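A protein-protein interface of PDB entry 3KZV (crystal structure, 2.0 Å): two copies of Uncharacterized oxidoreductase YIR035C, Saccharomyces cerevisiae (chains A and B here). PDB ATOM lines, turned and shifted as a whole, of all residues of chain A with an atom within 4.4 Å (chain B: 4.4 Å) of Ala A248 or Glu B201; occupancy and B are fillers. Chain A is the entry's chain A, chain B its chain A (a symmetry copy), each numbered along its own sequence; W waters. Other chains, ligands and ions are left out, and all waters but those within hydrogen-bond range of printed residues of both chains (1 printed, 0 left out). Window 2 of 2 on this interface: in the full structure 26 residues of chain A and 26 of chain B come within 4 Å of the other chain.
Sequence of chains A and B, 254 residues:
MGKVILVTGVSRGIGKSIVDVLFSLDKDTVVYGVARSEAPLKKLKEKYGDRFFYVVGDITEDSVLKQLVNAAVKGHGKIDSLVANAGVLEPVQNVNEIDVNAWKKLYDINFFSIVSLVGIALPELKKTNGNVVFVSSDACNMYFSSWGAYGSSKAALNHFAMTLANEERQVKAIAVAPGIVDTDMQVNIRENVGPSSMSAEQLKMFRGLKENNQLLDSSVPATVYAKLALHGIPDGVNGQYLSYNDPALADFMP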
ATOM      1  N   VAL A 237      15.871  14.889  -9.841  1.00  0.00           N
ATOM      2  CA  VAL A 237      16.280  16.241  -9.415  1.00  0.00           C
ATOM      3  C   VAL A 237      15.801  16.639  -8.002  1.00  0.00           C
ATOM      4  O   VAL A 237      15.902  17.808  -7.634  1.00  0.00           O
ATOM      5  CB  VAL A 237      15.917  17.416 -10.436  1.00  0.00           C
ATOM      6  CG1 VAL A 237      16.650  17.254 -11.759  1.00  0.00           C
ATOM      7  CG2 VAL A 237      14.387  17.518 -10.679  1.00  0.00           C
ATOM      8  N   LEU A 242      19.078  24.217  -9.520  1.00  0.00           N
ATOM      9  CA  LEU A 242      19.340  24.129 -10.985  1.00  0.00           C
ATOM     10  C   LEU A 242      18.856  25.464 -11.561  1.00  0.00           C
ATOM     11  O   LEU A 242      17.937  26.085 -10.983  1.00  0.00           O
ATOM     12  CB  LEU A 242      18.438  23.057 -11.653  1.00  0.00           C
ATOM     13  CG  LEU A 242      18.465  21.575 -11.374  1.00  0.00           C
ATOM     14  CD1 LEU A 242      17.563  20.851 -12.319  1.00  0.00           C
ATOM     15  CD2 LEU A 242      19.830  21.195 -11.680  1.00  0.00           C
ATOM     16  N   ASP A 246      18.302  24.163 -17.147  1.00  0.00           N
ATOM     17  CA  ASP A 246      19.121  22.942 -17.127  1.00  0.00           C
ATOM     18  C   ASP A 246      18.393  21.835 -17.942  1.00  0.00           C
ATOM     19  O   ASP A 246      17.156  21.678 -17.848  1.00  0.00           O
ATOM     20  CB  ASP A 246      19.391  22.455 -15.707  1.00  0.00           C
ATOM     21  CG  ASP A 246      20.316  21.276 -15.694  1.00  0.00           C
ATOM     22  OD1 ASP A 246      21.543  21.457 -15.938  1.00  0.00           O
ATOM     23  OD2 ASP A 246      19.747  20.178 -15.653  1.00  0.00           O
ATOM     24  N   PRO A 247      19.120  21.050 -18.729  1.00  0.00           N
ATOM     25  CA  PRO A 247      18.394  20.075 -19.539  1.00  0.00           C
ATOM     26  C   PRO A 247      17.504  19.098 -18.740  1.00  0.00           C
ATOM     27  O   PRO A 247      16.518  18.597 -19.268  1.00  0.00           O
ATOM     28  CB  PRO A 247      19.509  19.310 -20.245  1.00  0.00           C
ATOM     29  CG  PRO A 247      20.558  20.357 -20.497  1.00  0.00           C
ATOM     30  CD  PRO A 247      20.526  21.190 -19.175  1.00  0.00           C
ATOM     31  N   ALA A 248      17.832  18.843 -17.487  1.00  0.00           N
ATOM     32  CA  ALA A 248      16.996  17.913 -16.657  1.00  0.00           C
ATOM     33  C   ALA A 248      15.578  18.491 -16.501  1.00  0.00           C
ATOM     34  O   ALA A 248      14.632  17.772 -16.123  1.00  0.00           O
ATOM     35  CB  ALA A 248      17.682  17.634 -15.225  1.00  0.00           C
ATOM     36  N   LEU A 249      15.426  19.782 -16.807  1.00  0.00           N
ATOM     37  CA  LEU A 249      14.096  20.435 -16.758  1.00  0.00           C
ATOM     38  C   LEU A 249      13.408  20.639 -18.145  1.00  0.00           C
ATOM     39  O   LEU A 249      12.339  21.253 -18.208  1.00  0.00           O
ATOM     40  CB  LEU A 249      14.173  21.774 -15.999  1.00  0.00           C
ATOM     41  CG  LEU A 249      14.713  21.642 -14.540  1.00  0.00           C
ATOM     42  CD1 LEU A 249      14.786  23.022 -13.780  1.00  0.00           C
ATOM     43  CD2 LEU A 249      13.925  20.620 -13.719  1.00  0.00           C
ATOM     44  N   ALA A 250      14.004  20.120 -19.223  1.00  0.00           N
ATOM     45  CA  ALA A 250      13.390  20.219 -20.590  1.00  0.00           C
ATOM     46  C   ALA A 250      11.857  19.963 -20.629  1.00  0.00           C
ATOM     47  O   ALA A 250      11.157  20.632 -21.356  1.00  0.00           O
ATOM     48  CB  ALA A 250      14.147  19.273 -21.648  1.00  0.00           C
ATOM     49  N   SER B 146      23.272  19.369 -16.210  1.00  0.00           N
ATOM     50  CA  SER B 146      23.059  18.227 -17.103  1.00  0.00           C
ATOM     51  C   SER B 146      23.545  18.532 -18.520  1.00  0.00           C
ATOM     52  O   SER B 146      23.156  17.823 -19.479  1.00  0.00           O
ATOM     53  CB  SER B 146      21.595  17.935 -17.186  1.00  0.00           C
ATOM     54  OG  SER B 146      21.173  17.373 -15.991  1.00  0.00           O
ATOM     55  N   SER B 199      22.073  14.461 -25.607  1.00  0.00           N
ATOM     56  CA  SER B 199      20.942  13.662 -25.132  1.00  0.00           C
ATOM     57  C   SER B 199      19.625  14.286 -25.628  1.00  0.00           C
ATOM     58  O   SER B 199      19.573  15.437 -26.039  1.00  0.00           O
ATOM     59  CB  SER B 199      20.939  13.577 -23.628  1.00  0.00           C
ATOM     60  OG  SER B 199      20.660  14.902 -23.146  1.00  0.00           O
ATOM     61  N   ALA B 200      18.545  13.530 -25.555  1.00  0.00           N
ATOM     62  CA  ALA B 200      17.244  14.058 -25.959  1.00  0.00           C
ATOM     63  C   ALA B 200      16.888  15.334 -25.178  1.00  0.00           C
ATOM     64  O   ALA B 200      16.371  16.312 -25.725  1.00  0.00           O
ATOM     65  CB  ALA B 200      16.184  12.987 -25.744  1.00  0.00           C
ATOM     66  N   GLU B 201      17.182  15.316 -23.891  1.00  0.00           N
ATOM     67  CA  GLU B 201      16.963  16.487 -23.018  1.00  0.00           C
ATOM     68  C   GLU B 201      17.814  17.656 -23.405  1.00  0.00           C
ATOM     69  O   GLU B 201      17.354  18.823 -23.433  1.00  0.00           O
ATOM     70  CB  GLU B 201      17.246  16.077 -21.548  1.00  0.00           C
ATOM     71  CG  GLU B 201      16.076  15.274 -21.134  1.00  0.00           C
ATOM     72  CD  GLU B 201      16.030  15.007 -19.641  1.00  0.00           C
ATOM     73  OE1 GLU B 201      17.133  15.019 -18.996  1.00  0.00           O
ATOM     74  OE2 GLU B 201      14.865  14.834 -19.155  1.00  0.00           O
ATOM     75  N   GLN B 202      19.070  17.387 -23.691  1.00  0.00           N
ATOM     76  CA  GLN B 202      19.924  18.504 -24.105  1.00  0.00           C
ATOM     77  C   GLN B 202      19.436  19.140 -25.377  1.00  0.00           C
ATOM     78  O   GLN B 202      19.402  20.357 -25.464  1.00  0.00           O
ATOM     79  CB  GLN B 202      21.380  18.126 -24.272  1.00  0.00           C
ATOM     80  CG  GLN B 202      22.091  17.852 -22.903  1.00  0.00           C
ATOM     81  CD  GLN B 202      23.348  17.042 -23.097  1.00  0.00           C
ATOM     82  OE1 GLN B 202      23.633  16.584 -24.229  1.00  0.00           O
ATOM     83  NE2 GLN B 202      24.068  16.781 -21.999  1.00  0.00           N
ATOM     84  N   LEU B 203      19.080  18.307 -26.374  1.00  0.00           N
ATOM     85  CA  LEU B 203      18.576  18.790 -27.647  1.00  0.00           C
ATOM     86  C   LEU B 203      17.268  19.557 -27.481  1.00  0.00           C
ATOM     87  O   LEU B 203      17.072  20.623 -28.121  1.00  0.00           O
ATOM     88  CB  LEU B 203      18.407  17.591 -28.592  1.00  0.00           C
ATOM     89  CG  LEU B 203      17.965  17.914 -30.048  1.00  0.00           C
ATOM     90  CD1 LEU B 203      19.042  18.764 -30.739  1.00  0.00           C
ATOM     91  CD2 LEU B 203      17.653  16.588 -30.785  1.00  0.00           C
ATOM     92  N   LYS B 204      16.326  19.018 -26.685  1.00  0.00           N
ATOM     93  CA  LYS B 204      15.072  19.690 -26.511  1.00  0.00           C
ATOM     94  C   LYS B 204      15.277  21.083 -25.825  1.00  0.00           C
ATOM     95  O   LYS B 204      14.713  22.090 -26.263  1.00  0.00           O
ATOM     96  CB  LYS B 204      14.141  18.836 -25.651  1.00  0.00           C
ATOM     97  CG  LYS B 204      12.799  19.462 -25.434  1.00  0.00           C
ATOM     98  CD  LYS B 204      11.866  18.568 -24.667  1.00  0.00           C
ATOM     99  CE  LYS B 204      10.533  19.350 -24.465  1.00  0.00           C
ATOM    100  NZ  LYS B 204       9.514  18.374 -23.920  1.00  0.00           N
ATOM    101  N   MET B 205      16.116  21.156 -24.789  1.00  0.00           N
ATOM    102  CA  MET B 205      16.401  22.478 -24.137  1.00  0.00           C
ATOM    103  C   MET B 205      17.116  23.415 -25.107  1.00  0.00           C
ATOM    104  O   MET B 205      16.800  24.618 -25.232  1.00  0.00           O
ATOM    105  CB  MET B 205      17.261  22.298 -22.848  1.00  0.00           C
ATOM    106  CG  MET B 205      17.553  23.729 -22.124  1.00  0.00           C
ATOM    107  SD  MET B 205      15.967  24.540 -21.583  1.00  0.00           S
ATOM    108  CE  MET B 205      15.422  23.486 -20.233  1.00  0.00           C
HETATM  109  O   HOH W   1      12.780  17.213 -17.900  1.00  0.00           O
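The side-chain carboxylate of Asp A246 lies within hydrogen-bond range of the backbone NH of Ser B146 (2.7 Å).
The side-chain carboxylate of Asp A246 sits at hydrogen-bond distance from the backbone NH of Ala A248. The backbone carbonyl oxygen (O) of Ser B146 lies within hydrogen-bond range of the side-chain amide nitrogen (NE2) of Gln B202 (2.9 Å). The backbone NH (N) of Ser B199 sits at hydrogen-bond distance from the side-chain amide oxygen (OE1) of Gln B202.
Among the printed residues, pairs that only touch across the chains: Asp A246 with Met B205 (3.5 Å), Pro A247 with Ser B146 (3.8 Å), Pro A247 with Glu B201 (3.5 Å), Pro A247 with Gln B202 (3.8 Å), Ala A248 with Ser B146 (3.6 Å), Ala A248 with Glu B201 (3.7 Å), Ala A250 with Glu B201 (3.7 Å), Ala A250 with Lys B204 (3.4 Å) and Ala A250 with Met B205 (3.8 Å).
Ala A248 touches just these residues of chain B: Ser B146 and Glu B201. Glu B201 touches just these residues of chain A: Pro A247, Ala A248 and Ala A250. Printed residues of chain A within 4 Å of Gln B202: Pro A247 (3.8 Å). Of the printed residues of chain A, Ser B146 touches Asp A246 (2.7 Å), Pro A247 (3.8 Å) and Ala A248 (3.6 Å). Of the printed residues of chain B, Ala A250 touches Glu B201, Lys B204 and Met B205. Of the printed residues of chain B, Pro A247 touches Ser B146, Glu B201 and Gln B202. Printed residues of chain A within 4 Å of Lys B204: Ala A250 (3.4 Å). The nearest printed residue of chain A that does not touch Glu B201 is Leu A249 (5.5 Å). The nearest printed residue of chain A that does not touch Gln B202 is Ala A250 (5.7 Å).
Printed residues of chain A that touch a printed residue of chain B: Asp A246, Pro A247, Ala A248 and Ala A250. Hydrophobic or aromatic side chains of chain A within 4 Å of the printed part of chain B: Pro A247, Ala A248 and Ala A250. Among the printed residues, no Asp or Glu carboxylate lies within 4 Å of a Lys or Arg side-chain nitrogen of the other chain.
No position is printed for both chains. Of the 10 pairs that touch across the chains among the printed residues, none has its exchanged pair printed and touching as well.
Water W1 lies within hydrogen-bond range of O of Ala A248 (2.6 Å), OE2 of Glu B201 (3.4 Å) and N of Ala A250 (3.4 Å).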
